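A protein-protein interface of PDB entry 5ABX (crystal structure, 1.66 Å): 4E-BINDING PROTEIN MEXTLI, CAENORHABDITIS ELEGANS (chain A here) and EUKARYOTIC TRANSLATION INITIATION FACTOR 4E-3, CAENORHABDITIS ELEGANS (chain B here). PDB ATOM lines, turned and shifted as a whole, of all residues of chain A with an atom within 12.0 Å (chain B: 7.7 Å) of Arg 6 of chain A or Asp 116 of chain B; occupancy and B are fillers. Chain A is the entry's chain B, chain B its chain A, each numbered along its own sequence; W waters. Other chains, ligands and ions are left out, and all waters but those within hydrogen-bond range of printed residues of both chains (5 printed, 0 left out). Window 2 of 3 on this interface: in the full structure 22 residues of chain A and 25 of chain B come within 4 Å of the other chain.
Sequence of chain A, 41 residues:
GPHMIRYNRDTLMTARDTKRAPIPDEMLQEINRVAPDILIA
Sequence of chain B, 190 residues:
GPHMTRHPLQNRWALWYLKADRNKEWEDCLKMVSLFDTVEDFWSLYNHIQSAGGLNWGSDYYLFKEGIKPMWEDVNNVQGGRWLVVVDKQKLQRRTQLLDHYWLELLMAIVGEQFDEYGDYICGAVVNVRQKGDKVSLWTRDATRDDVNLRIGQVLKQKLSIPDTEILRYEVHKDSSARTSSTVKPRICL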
ATOM      1  N   GLY A   1      14.176  20.337 -10.817  1.00  0.00           N
ATOM      2  CA  GLY A   1      12.993  19.762 -11.429  1.00  0.00           C
ATOM      3  C   GLY A   1      11.927  20.814 -11.687  1.00  0.00           C
ATOM      4  O   GLY A   1      12.089  21.980 -11.311  1.00  0.00           O
ATOM      5  N   PRO A   2      10.826  20.407 -12.335  1.00  0.00           N
ATOM      6  CA  PRO A   2       9.727  21.317 -12.690  1.00  0.00           C
ATOM      7  C   PRO A   2       8.824  21.691 -11.508  1.00  0.00           C
ATOM      8  O   PRO A   2       8.920  21.083 -10.444  1.00  0.00           O
ATOM      9  CB  PRO A   2       8.947  20.522 -13.746  1.00  0.00           C
ATOM     10  CG  PRO A   2       9.216  19.090 -13.420  1.00  0.00           C
ATOM     11  CD  PRO A   2      10.605  19.036 -12.838  1.00  0.00           C
ATOM     12  N   HIS A   3       7.971  22.695 -11.708  1.00  0.00           N
ATOM     13  CA  HIS A   3       6.963  23.096 -10.724  1.00  0.00           C
ATOM     14  C   HIS A   3       5.766  22.146 -10.724  1.00  0.00           C
ATOM     15  O   HIS A   3       5.562  21.393 -11.678  1.00  0.00           O
ATOM     16  CB  HIS A   3       6.445  24.516 -11.009  1.00  0.00           C
ATOM     17  CG  HIS A   3       7.484  25.589 -10.896  1.00  0.00           C
ATOM     18  ND1 HIS A   3       8.192  26.058 -11.982  1.00  0.00           N
ATOM     19  CD2 HIS A   3       7.915  26.303  -9.828  1.00  0.00           C
ATOM     20  CE1 HIS A   3       9.025  27.005 -11.587  1.00  0.00           C
ATOM     21  NE2 HIS A   3       8.877  27.173 -10.284  1.00  0.00           N
ATOM     22  N   MET A   4       4.987  22.200  -9.650  1.00  0.00           N
ATOM     23  CA  MET A   4       3.664  21.585  -9.597  1.00  0.00           C
ATOM     24  C   MET A   4       2.858  21.995 -10.818  1.00  0.00           C
ATOM     25  O   MET A   4       2.942  23.140 -11.257  1.00  0.00           O
ATOM     26  CB  MET A   4       2.928  22.012  -8.324  1.00  0.00           C
ATOM     27  CG  MET A   4       3.546  21.527  -7.031  1.00  0.00           C
ATOM     28  SD  MET A   4       3.247  19.773  -6.776  1.00  0.00           S
ATOM     29  CE  MET A   4       4.727  19.060  -7.492  1.00  0.00           C
ATOM     30  N   ILE A   5       2.081  21.067 -11.372  1.00  0.00           N
ATOM     31  CA  ILE A   5       1.193  21.394 -12.474  1.00  0.00           C
ATOM     32  C   ILE A   5      -0.153  21.753 -11.879  1.00  0.00           C
ATOM     33  O   ILE A   5      -0.753  20.957 -11.157  1.00  0.00           O
ATOM     34  CB  ILE A   5       1.029  20.242 -13.468  1.00  0.00           C
ATOM     35  CG1 ILE A   5       2.399  19.778 -13.968  1.00  0.00           C
ATOM     36  CG2 ILE A   5       0.190  20.692 -14.654  1.00  0.00           C
ATOM     37  CD1 ILE A   5       2.491  18.299 -14.151  1.00  0.00           C
ATOM     38  N   ARG A   6      -0.594  22.972 -12.159  1.00  0.00           N
ATOM     39  CA  ARG A   6      -1.854  23.480 -11.643  1.00  0.00           C
ATOM     40  C   ARG A   6      -2.745  23.936 -12.781  1.00  0.00           C
ATOM     41  O   ARG A   6      -2.262  24.378 -13.822  1.00  0.00           O
ATOM     42  CB  ARG A   6      -1.612  24.646 -10.681  1.00  0.00           C
ATOM     43  CG  ARG A   6      -0.605  24.337  -9.600  1.00  0.00           C
ATOM     44  CD  ARG A   6      -0.549  25.451  -8.593  1.00  0.00           C
ATOM     45  NE  ARG A   6       0.619  25.347  -7.726  1.00  0.00           N
ATOM     46  CZ  ARG A   6       0.663  24.676  -6.579  1.00  0.00           C
ATOM     47  NH1 ARG A   6      -0.397  24.014  -6.128  1.00  0.00           N
ATOM     48  NH2 ARG A   6       1.783  24.669  -5.871  1.00  0.00           N
ATOM     49  N   TYR A   7      -4.052  23.845 -12.557  1.00  0.00           N
ATOM     50  CA  TYR A   7      -5.040  24.346 -13.497  1.00  0.00           C
ATOM     51  C   TYR A   7      -6.080  25.096 -12.689  1.00  0.00           C
ATOM     52  O   TYR A   7      -6.762  24.507 -11.860  1.00  0.00           O
ATOM     53  CB  TYR A   7      -5.718  23.223 -14.288  1.00  0.00           C
ATOM     54  CG  TYR A   7      -4.778  22.368 -15.101  1.00  0.00           C
ATOM     55  CD1 TYR A   7      -4.157  21.257 -14.542  1.00  0.00           C
ATOM     56  CD2 TYR A   7      -4.524  22.667 -16.432  1.00  0.00           C
ATOM     57  CE1 TYR A   7      -3.300  20.471 -15.288  1.00  0.00           C
ATOM     58  CE2 TYR A   7      -3.678  21.894 -17.182  1.00  0.00           C
ATOM     59  CZ  TYR A   7      -3.060  20.800 -16.607  1.00  0.00           C
ATOM     60  OH  TYR A   7      -2.209  20.034 -17.366  1.00  0.00           O
ATOM     61  N   ASN A   8      -6.201  26.397 -12.911  1.00  0.00           N
ATOM     62  CA  ASN A   8      -7.243  27.118 -12.217  1.00  0.00           C
ATOM     63  C   ASN A   8      -8.581  26.817 -12.884  1.00  0.00           C
ATOM     64  O   ASN A   8      -8.639  26.188 -13.946  1.00  0.00           O
ATOM     65  CB  ASN A   8      -6.943  28.624 -12.161  1.00  0.00           C
ATOM     66  CG  ASN A   8      -6.975  29.299 -13.509  1.00  0.00           C
ATOM     67  OD1 ASN A   8      -7.749  28.946 -14.394  1.00  0.00           O
ATOM     68  ND2 ASN A   8      -6.134  30.317 -13.661  1.00  0.00           N
ATOM     69  N   ARG A   9      -9.648  27.257 -12.234  1.00  0.00           N
ATOM     70  CA  ARG A   9     -11.004  26.970 -12.658  1.00  0.00           C
ATOM     71  C   ARG A   9     -11.293  27.363 -14.107  1.00  0.00           C
ATOM     72  O   ARG A   9     -11.908  26.598 -14.851  1.00  0.00           O
ATOM     73  CB  ARG A   9     -11.971  27.692 -11.729  1.00  0.00           C
ATOM     74  CG  ARG A   9     -13.416  27.410 -12.011  1.00  0.00           C
ATOM     75  CD  ARG A   9     -14.271  28.182 -11.050  1.00  0.00           C
ATOM     76  NE  ARG A   9     -15.661  27.753 -11.101  1.00  0.00           N
ATOM     77  CZ  ARG A   9     -16.547  28.178 -11.992  1.00  0.00           C
ATOM     78  NH1 ARG A   9     -16.193  29.044 -12.936  1.00  0.00           N
ATOM     79  NH2 ARG A   9     -17.789  27.721 -11.944  1.00  0.00           N
ATOM     80  N   ASP A  10     -10.873  28.561 -14.500  1.00  0.00           N
ATOM     81  CA  ASP A  10     -11.104  29.024 -15.868  1.00  0.00           C
ATOM     82  C   ASP A  10     -10.437  28.115 -16.895  1.00  0.00           C
ATOM     83  O   ASP A  10     -11.016  27.820 -17.938  1.00  0.00           O
ATOM     84  CB  ASP A  10     -10.593  30.459 -16.055  1.00  0.00           C
ATOM     85  CG  ASP A  10     -11.369  31.471 -15.227  1.00  0.00           C
ATOM     86  OD1 ASP A  10     -12.618  31.439 -15.262  1.00  0.00           O
ATOM     87  OD2 ASP A  10     -10.730  32.301 -14.543  1.00  0.00           O
ATOM     88  N   THR A  11      -9.215  27.677 -16.606  1.00  0.00           N
ATOM     89  CA  THR A  11      -8.486  26.837 -17.546  1.00  0.00           C
ATOM     90  C   THR A  11      -9.193  25.490 -17.703  1.00  0.00           C
ATOM     91  O   THR A  11      -9.340  24.989 -18.816  1.00  0.00           O
ATOM     92  CB  THR A  11      -7.023  26.626 -17.098  1.00  0.00           C
ATOM     93  OG1 THR A  11      -6.359  27.896 -17.042  1.00  0.00           O
ATOM     94  CG2 THR A  11      -6.268  25.722 -18.064  1.00  0.00           C
ATOM     95  N   LEU A  12      -9.646  24.912 -16.596  1.00  0.00           N
ATOM     96  CA  LEU A  12     -10.342  23.631 -16.670  1.00  0.00           C
ATOM     97  C   LEU A  12     -11.663  23.762 -17.406  1.00  0.00           C
ATOM     98  O   LEU A  12     -12.036  22.889 -18.186  1.00  0.00           O
ATOM     99  CB  LEU A  12     -10.599  23.055 -15.276  1.00  0.00           C
ATOM    100  CG  LEU A  12      -9.406  22.537 -14.485  1.00  0.00           C
ATOM    101  CD1 LEU A  12      -9.867  21.938 -13.167  1.00  0.00           C
ATOM    102  CD2 LEU A  12      -8.617  21.504 -15.268  1.00  0.00           C
ATOM    103  N   MET A  13     -12.391  24.842 -17.148  1.00  0.00           N
ATOM    104  CA  MET A  13     -13.700  25.029 -17.764  1.00  0.00           C
ATOM    105  C   MET A  13     -13.587  25.252 -19.269  1.00  0.00           C
ATOM    106  O   MET A  13     -14.426  24.778 -20.034  1.00  0.00           O
ATOM    107  CB  MET A  13     -14.430  26.210 -17.118  1.00  0.00           C
ATOM    108  CG  MET A  13     -14.928  25.930 -15.712  1.00  0.00           C
ATOM    109  SD  MET A  13     -16.333  24.799 -15.669  1.00  0.00           S
ATOM    110  CE  MET A  13     -17.648  25.868 -16.250  1.00  0.00           C
ATOM    111  N   THR A  14     -12.551  25.962 -19.702  1.00  0.00           N
ATOM    112  CA  THR A  14     -12.348  26.196 -21.126  1.00  0.00           C
ATOM    113  C   THR A  14     -11.979  24.891 -21.826  1.00  0.00           C
ATOM    114  O   THR A  14     -12.319  24.681 -22.990  1.00  0.00           O
ATOM    115  CB  THR A  14     -11.247  27.241 -21.375  1.00  0.00           C
ATOM    116  OG1 THR A  14     -11.589  28.465 -20.716  1.00  0.00           O
ATOM    117  CG2 THR A  14     -11.075  27.507 -22.863  1.00  0.00           C
ATOM    118  N   ALA A  15     -11.289  24.011 -21.106  1.00  0.00           N
ATOM    119  CA  ALA A  15     -10.825  22.751 -21.680  1.00  0.00           C
ATOM    120  C   ALA A  15     -11.949  21.730 -21.779  1.00  0.00           C
ATOM    121  O   ALA A  15     -11.810  20.713 -22.448  1.00  0.00           O
ATOM    122  CB  ALA A  15      -9.677  22.184 -20.854  1.00  0.00           C
ATOM    123  N   PRO B   8      -1.690  16.881 -18.717  1.00  0.00           N
ATOM    124  CA  PRO B   8      -1.540  16.006 -17.551  1.00  0.00           C
ATOM    125  C   PRO B   8      -1.864  16.674 -16.239  1.00  0.00           C
ATOM    126  O   PRO B   8      -1.580  17.860 -16.058  1.00  0.00           O
ATOM    127  CB  PRO B   8      -0.055  15.633 -17.580  1.00  0.00           C
ATOM    128  CG  PRO B   8       0.573  16.720 -18.324  1.00  0.00           C
ATOM    129  CD  PRO B   8      -0.397  17.130 -19.371  1.00  0.00           C
ATOM    130  N   LEU B   9      -2.459  15.908 -15.334  1.00  0.00           N
ATOM    131  CA  LEU B   9      -2.660  16.345 -13.963  1.00  0.00           C
ATOM    132  C   LEU B   9      -1.428  16.012 -13.121  1.00  0.00           C
ATOM    133  O   LEU B   9      -0.658  15.107 -13.451  1.00  0.00           O
ATOM    134  CB  LEU B   9      -3.895  15.675 -13.367  1.00  0.00           C
ATOM    135  CG  LEU B   9      -5.202  15.883 -14.125  1.00  0.00           C
ATOM    136  CD1 LEU B   9      -6.297  15.009 -13.544  1.00  0.00           C
ATOM    137  CD2 LEU B   9      -5.618  17.357 -14.052  1.00  0.00           C
ATOM    138  N   GLN B  10      -1.249  16.740 -12.028  1.00  0.00           N
ATOM    139  CA  GLN B  10      -0.148  16.479 -11.118  1.00  0.00           C
ATOM    140  C   GLN B  10      -0.267  15.080 -10.536  1.00  0.00           C
ATOM    141  O   GLN B  10       0.715  14.347 -10.430  1.00  0.00           O
ATOM    142  CB  GLN B  10      -0.123  17.525 -10.006  1.00  0.00           C
ATOM    143  CG  GLN B  10       1.014  17.338  -9.018  1.00  0.00           C
ATOM    144  CD  GLN B  10       2.382  17.477  -9.675  1.00  0.00           C
ATOM    145  OE1 GLN B  10       2.589  18.342 -10.524  1.00  0.00           O
ATOM    146  NE2 GLN B  10       3.306  16.597  -9.309  1.00  0.00           N
ATOM    147  N   VAL B  39      -6.626  16.238 -17.808  1.00  0.00           N
ATOM    148  CA  VAL B  39      -7.811  17.083 -17.809  1.00  0.00           C
ATOM    149  C   VAL B  39      -8.864  16.499 -18.745  1.00  0.00           C
ATOM    150  O   VAL B  39     -10.047  16.472 -18.415  1.00  0.00           O
ATOM    151  CB  VAL B  39      -7.465  18.519 -18.232  1.00  0.00           C
ATOM    152  CG1 VAL B  39      -8.720  19.369 -18.389  1.00  0.00           C
ATOM    153  CG2 VAL B  39      -6.532  19.148 -17.214  1.00  0.00           C
ATOM    154  N   ALA B 109     -11.024  21.973  -7.923  1.00  0.00           N
ATOM    155  CA  ALA B 109     -10.002  22.512  -7.034  1.00  0.00           C
ATOM    156  C   ALA B 109      -8.954  21.458  -6.697  1.00  0.00           C
ATOM    157  O   ALA B 109      -7.769  21.760  -6.621  1.00  0.00           O
ATOM    158  CB  ALA B 109     -10.625  23.055  -5.750  1.00  0.00           C
ATOM    159  N   VAL B 111      -8.202  18.418  -8.458  1.00  0.00           N
ATOM    160  CA  VAL B 111      -7.413  17.922  -9.598  1.00  0.00           C
ATOM    161  C   VAL B 111      -6.563  19.031 -10.209  1.00  0.00           C
ATOM    162  O   VAL B 111      -5.490  18.762 -10.764  1.00  0.00           O
ATOM    163  CB  VAL B 111      -8.279  17.266 -10.718  1.00  0.00           C
ATOM    164  CG1 VAL B 111      -9.116  16.152 -10.129  1.00  0.00           C
ATOM    165  CG2 VAL B 111      -9.135  18.271 -11.464  1.00  0.00           C
ATOM    166  N   GLY B 112      -7.015  20.275 -10.071  1.00  0.00           N
ATOM    167  CA  GLY B 112      -6.243  21.422 -10.513  1.00  0.00           C
ATOM    168  C   GLY B 112      -5.172  21.877  -9.529  1.00  0.00           C
ATOM    169  O   GLY B 112      -4.480  22.857  -9.795  1.00  0.00           O
ATOM    170  N   GLU B 113      -5.047  21.178  -8.404  1.00  0.00           N
ATOM    171  CA  GLU B 113      -4.026  21.451  -7.383  1.00  0.00           C
ATOM    172  C   GLU B 113      -4.099  22.899  -6.896  1.00  0.00           C
ATOM    173  O   GLU B 113      -3.104  23.629  -6.888  1.00  0.00           O
ATOM    174  CB  GLU B 113      -2.620  21.136  -7.928  1.00  0.00           C
ATOM    175  CG  GLU B 113      -2.446  19.690  -8.413  1.00  0.00           C
ATOM    176  CD  GLU B 113      -2.389  18.669  -7.285  1.00  0.00           C
ATOM    177  OE1 GLU B 113      -1.882  19.000  -6.190  1.00  0.00           O
ATOM    178  OE2 GLU B 113      -2.841  17.517  -7.490  1.00  0.00           O
ATOM    179  N   GLN B 114      -5.290  23.299  -6.468  1.00  0.00           N
ATOM    180  CA  GLN B 114      -5.548  24.683  -6.090  1.00  0.00           C
ATOM    181  C   GLN B 114      -5.381  24.946  -4.598  1.00  0.00           C
ATOM    182  O   GLN B 114      -5.771  26.010  -4.106  1.00  0.00           O
ATOM    183  CB  GLN B 114      -6.968  25.072  -6.524  1.00  0.00           C
ATOM    184  CG  GLN B 114      -7.143  25.111  -8.027  1.00  0.00           C
ATOM    185  CD  GLN B 114      -6.311  26.207  -8.661  1.00  0.00           C
ATOM    186  OE1 GLN B 114      -6.634  27.389  -8.543  1.00  0.00           O
ATOM    187  NE2 GLN B 114      -5.220  25.825  -9.315  1.00  0.00           N
ATOM    188  N   PHE B 115      -4.790  24.000  -3.875  1.00  0.00           N
ATOM    189  CA  PHE B 115      -4.592  24.165  -2.445  1.00  0.00           C
ATOM    190  C   PHE B 115      -3.139  24.562  -2.133  1.00  0.00           C
ATOM    191  O   PHE B 115      -2.578  24.187  -1.106  1.00  0.00           O
ATOM    192  CB  PHE B 115      -5.027  22.893  -1.712  1.00  0.00           C
ATOM    193  CG  PHE B 115      -6.508  22.658  -1.783  1.00  0.00           C
ATOM    194  CD1 PHE B 115      -7.070  21.967  -2.845  1.00  0.00           C
ATOM    195  CD2 PHE B 115      -7.349  23.181  -0.816  1.00  0.00           C
ATOM    196  CE1 PHE B 115      -8.438  21.772  -2.920  1.00  0.00           C
ATOM    197  CE2 PHE B 115      -8.719  22.994  -0.882  1.00  0.00           C
ATOM    198  CZ  PHE B 115      -9.267  22.290  -1.933  1.00  0.00           C
ATOM    199  N   ASP B 116      -2.560  25.342  -3.044  1.00  0.00           N
ATOM    200  CA  ASP B 116      -1.266  25.989  -2.832  1.00  0.00           C
ATOM    201  C   ASP B 116      -0.184  24.979  -2.451  1.00  0.00           C
ATOM    202  O   ASP B 116       0.014  23.984  -3.144  1.00  0.00           O
ATOM    203  CB  ASP B 116      -1.394  27.075  -1.757  1.00  0.00           C
ATOM    204  CG  ASP B 116      -2.461  28.106  -2.088  1.00  0.00           C
ATOM    205  OD1 ASP B 116      -2.519  28.563  -3.251  1.00  0.00           O
ATOM    206  OD2 ASP B 116      -3.243  28.462  -1.180  1.00  0.00           O
ATOM    207  N   GLU B 117       0.505  25.225  -1.342  1.00  0.00           N
ATOM    208  CA  GLU B 117       1.621  24.377  -0.942  1.00  0.00           C
ATOM    209  C   GLU B 117       1.178  23.168  -0.120  1.00  0.00           C
ATOM    210  O   GLU B 117       2.020  22.408   0.362  1.00  0.00           O
ATOM    211  CB  GLU B 117       2.652  25.189  -0.142  1.00  0.00           C
ATOM    212  CG  GLU B 117       2.118  25.832   1.136  1.00  0.00           C
ATOM    213  CD  GLU B 117       1.455  27.192   0.914  1.00  0.00           C
ATOM    214  OE1 GLU B 117       1.408  27.668  -0.242  1.00  0.00           O
ATOM    215  OE2 GLU B 117       0.980  27.789   1.906  1.00  0.00           O
ATOM    216  N   TYR B 118      -0.132  22.972   0.026  1.00  0.00           N
ATOM    217  CA  TYR B 118      -0.642  21.922   0.904  1.00  0.00           C
ATOM    218  C   TYR B 118      -1.282  20.763   0.148  1.00  0.00           C
ATOM    219  O   TYR B 118      -2.006  19.962   0.741  1.00  0.00           O
ATOM    220  CB  TYR B 118      -1.650  22.512   1.894  1.00  0.00           C
ATOM    221  CG  TYR B 118      -1.046  23.574   2.786  1.00  0.00           C
ATOM    222  CD1 TYR B 118       0.055  23.293   3.585  1.00  0.00           C
ATOM    223  CD2 TYR B 118      -1.569  24.856   2.823  1.00  0.00           C
ATOM    224  CE1 TYR B 118       0.615  24.266   4.401  1.00  0.00           C
ATOM    225  CE2 TYR B 118      -1.016  25.829   3.631  1.00  0.00           C
ATOM    226  CZ  TYR B 118       0.071  25.531   4.416  1.00  0.00           C
ATOM    227  OH  TYR B 118       0.606  26.517   5.217  1.00  0.00           O
ATOM    228  N   GLY B 119      -0.991  20.656  -1.145  1.00  0.00           N
ATOM    229  CA  GLY B 119      -1.550  19.599  -1.974  1.00  0.00           C
ATOM    230  C   GLY B 119      -1.223  18.190  -1.508  1.00  0.00           C
ATOM    231  O   GLY B 119      -2.029  17.272  -1.679  1.00  0.00           O
ATOM    232  N   ASP B 120      -0.044  17.998  -0.925  1.00  0.00           N
ATOM    233  CA  ASP B 120       0.344  16.675  -0.444  1.00  0.00           C
ATOM    234  C   ASP B 120      -0.529  16.197   0.715  1.00  0.00           C
ATOM    235  O   ASP B 120      -0.592  15.001   0.990  1.00  0.00           O
ATOM    236  CB  ASP B 120       1.815  16.669  -0.016  1.00  0.00           C
ATOM    237  CG  ASP B 120       2.769  16.716  -1.199  1.00  0.00           C
ATOM    238  OD1 ASP B 120       2.305  16.562  -2.352  1.00  0.00           O
ATOM    239  OD2 ASP B 120       3.986  16.893  -0.975  1.00  0.00           O
ATOM    240  N   ILE B 122      -3.797  16.614   0.819  1.00  0.00           N
ATOM    241  CA  ILE B 122      -5.108  16.253   0.277  1.00  0.00           C
ATOM    242  C   ILE B 122      -5.138  14.759  -0.011  1.00  0.00           C
ATOM    243  O   ILE B 122      -4.287  14.257  -0.735  1.00  0.00           O
ATOM    244  CB  ILE B 122      -5.429  17.013  -1.041  1.00  0.00           C
ATOM    245  CG1 ILE B 122      -5.324  18.538  -0.870  1.00  0.00           C
ATOM    246  CG2 ILE B 122      -6.803  16.618  -1.574  1.00  0.00           C
ATOM    247  CD1 ILE B 122      -6.468  19.177  -0.134  1.00  0.00           C
ATOM    248  N   ARG B 151      -5.894  26.373   6.440  1.00  0.00           N
ATOM    249  CA  ARG B 151      -5.686  26.953   5.119  1.00  0.00           C
ATOM    250  C   ARG B 151      -6.474  26.202   4.049  1.00  0.00           C
ATOM    251  O   ARG B 151      -7.046  26.816   3.151  1.00  0.00           O
ATOM    252  CB  ARG B 151      -4.207  26.963   4.745  1.00  0.00           C
ATOM    253  CG  ARG B 151      -3.932  27.552   3.364  1.00  0.00           C
ATOM    254  CD  ARG B 151      -4.558  28.930   3.190  1.00  0.00           C
ATOM    255  NE  ARG B 151      -4.230  29.518   1.892  1.00  0.00           N
ATOM    256  CZ  ARG B 151      -4.983  30.418   1.264  1.00  0.00           C
ATOM    257  NH1 ARG B 151      -6.121  30.832   1.808  1.00  0.00           N
ATOM    258  NH2 ARG B 151      -4.604  30.897   0.087  1.00  0.00           N
ATOM    259  N   ILE B 152      -6.488  24.878   4.144  1.00  0.00           N
ATOM    260  CA  ILE B 152      -7.251  24.053   3.212  1.00  0.00           C
ATOM    261  C   ILE B 152      -8.743  24.387   3.310  1.00  0.00           C
ATOM    262  O   ILE B 152      -9.432  24.469   2.293  1.00  0.00           O
ATOM    263  CB  ILE B 152      -6.997  22.550   3.481  1.00  0.00           C
ATOM    264  CG1 ILE B 152      -5.572  22.194   3.049  1.00  0.00           C
ATOM    265  CG2 ILE B 152      -8.010  21.678   2.751  1.00  0.00           C
ATOM    266  CD1 ILE B 152      -5.103  20.776   3.443  1.00  0.00           C
ATOM    267  N   VAL B 155      -9.561  27.744   1.550  1.00  0.00           N
ATOM    268  CA  VAL B 155      -9.632  27.595   0.101  1.00  0.00           C
ATOM    269  C   VAL B 155     -10.938  26.897  -0.272  1.00  0.00           C
ATOM    270  O   VAL B 155     -11.603  27.286  -1.232  1.00  0.00           O
ATOM    271  CB  VAL B 155      -8.409  26.808  -0.440  1.00  0.00           C
ATOM    272  CG1 VAL B 155      -8.561  26.476  -1.922  1.00  0.00           C
ATOM    273  CG2 VAL B 155      -7.130  27.602  -0.202  1.00  0.00           C
HETATM  274  O   HOH W   1      -2.554  26.479  -5.706  1.00  0.00           O
HETATM  275  O   HOH W   2      -2.849  19.224 -11.926  1.00  0.00           O
HETATM  276  O   HOH W   3       4.928  18.586 -11.992  1.00  0.00           O
HETATM  277  O   HOH W   4      -9.210  28.896  -9.874  1.00  0.00           O
HETATM  278  O   HOH W   5      -0.854  21.248  -4.967  1.00  0.00           O
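The backbone carbonyl oxygen (O) of Pro 8 of chain B lies within hydrogen-bond range of the side-chain hydroxyl (OH) of Tyr 7 of chain A (2.6 Å).
The backbone NH of Ile 5 of chain A sits at hydrogen-bond distance from the side-chain amide oxygen of Gln 10 of chain B.
O of Gly 112 of chain B is in hydrogen-bond range of N of Tyr 7 of chain A, at 3.0 Å.
NH1 of Arg 6 of chain A sits at hydrogen-bond distance from O of Glu 113 of chain B (2.8 Å).
The side-chain amide nitrogen of Gln 114 of chain B lies within hydrogen-bond range of the backbone carbonyl oxygen of Tyr 7 of chain A (3.3 Å).
The backbone carbonyl oxygen (O) of Asp 116 of chain B is in hydrogen-bond range of the guanidinium group (NH1) of Arg 6 of chain A, at 3.0 Å.
N of Gln 114 of chain B is in hydrogen-bond range of O of Ala 109 of chain B (2.9 Å).
The backbone carbonyl oxygen (O) of Gly 112 of chain B sits at hydrogen-bond distance from the side-chain amide nitrogen (NE2) of Gln 114 of chain B, 3.1 Å away.
OD2 of Asp 116 of chain B lies within salt-bridge range of NH2 of Arg 151 of chain B (3.1 Å).
N of Asp 10 of chain A lies within hydrogen-bond range of OD1 of Asn 8 of chain A (3.1 Å).
The side-chain amide oxygen (OD1) of Asn 8 of chain A is in hydrogen-bond range of the backbone NH (N) of Thr 11 of chain A (2.9 Å).
Of the 15 printed residues of chain A, 7 touch a printed residue of chain B.
Hydrophobic or aromatic side chains of chain A within 4 Å of the printed part of chain B: Met 4, Ile 5, Tyr 7, Leu 12 and Ala 15.
Among the printed residues, no Asp or Glu carboxylate lies within 4 Å of a Lys or Arg side-chain nitrogen of the other chain.
Among the printed residues, pairs that only touch across the chains: Met 4 of chain A with Gln 10 of chain B (3.4 Å), Ile 5 of chain A with Pro 8 of chain B (3.6 Å), Ile 5 of chain A with Glu 113 of chain B (3.5 Å), Arg 6 of chain A with Gly 112 of chain B (3.3 Å), Tyr 7 of chain A with Val 39 of chain B (3.9 Å), Asn 8 of chain A with Gln 114 of chain B (3.7 Å), Leu 12 of chain A with Val 39 of chain B (3.7 Å) and Ala 15 of chain A with Val 39 of chain B (3.9 Å).
Arg 6 of chain A touches just these residues of chain B: Gly 112 (3.3 Å), Glu 113 (2.8 Å) and Asp 116 (3.0 Å).
Of the printed residues of chain B, Ala 15 of chain A touches Val 39 (3.9 Å).
Printed residues of chain A within 4 Å of Pro 8 of chain B: Ile 5 (3.6 Å) and Tyr 7 (2.6 Å).
Printed residues of chain A within 4 Å of Val 39 of chain B: Tyr 7 (3.9 Å), Leu 12 (3.7 Å) and Ala 15 (3.9 Å).
Gly 112 of chain B touches just these residues of chain A: Arg 6 and Tyr 7.
Of chain A, only Ile 5 (3.5 Å) and Arg 6 (2.8 Å) come within 4 Å of Glu 113 of chain B.
No residue of chain A comes within 4 Å of Phe 115 of chain B.
Printed residues of chain A within 4 Å of Asp 116 of chain B: Arg 6 (3.0 Å).
Tyr 118 of chain B touches none of the printed residues of chain A.
The nearest residue of chain B that does not touch Arg 6 of chain A is Gln 114 of chain B (4.03 Å).
Water W5 lies within hydrogen-bond range of OE1 of Glu 113 of chain B (2.8 Å), NH1 of Arg 6 of chain A (3.0 Å) and O of Asp 116 of chain B (3.4 Å).
Water W3 lies within hydrogen-bond range of OE1 of Gln 10 of chain B (2.8 Å) and O of His 3 of chain A (2.9 Å).
Water W2 lies within hydrogen-bond range of O of Ile 5 of chain A, O of Val 111 of chain B and N of Gln 10 of chain B.
Water W1 lies within hydrogen-bond range of N of Asp 116 of chain B (2.9 Å), O of Glu 113 of chain B (3.1 Å) and NH1 of Arg 6 of chain A (3.3 Å).
Water W4 lies within hydrogen-bond range of the backbone NH of Arg 9 of chain A (2.9 Å) and the side-chain amide oxygen of Gln 114 of chain B (3.3 Å).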
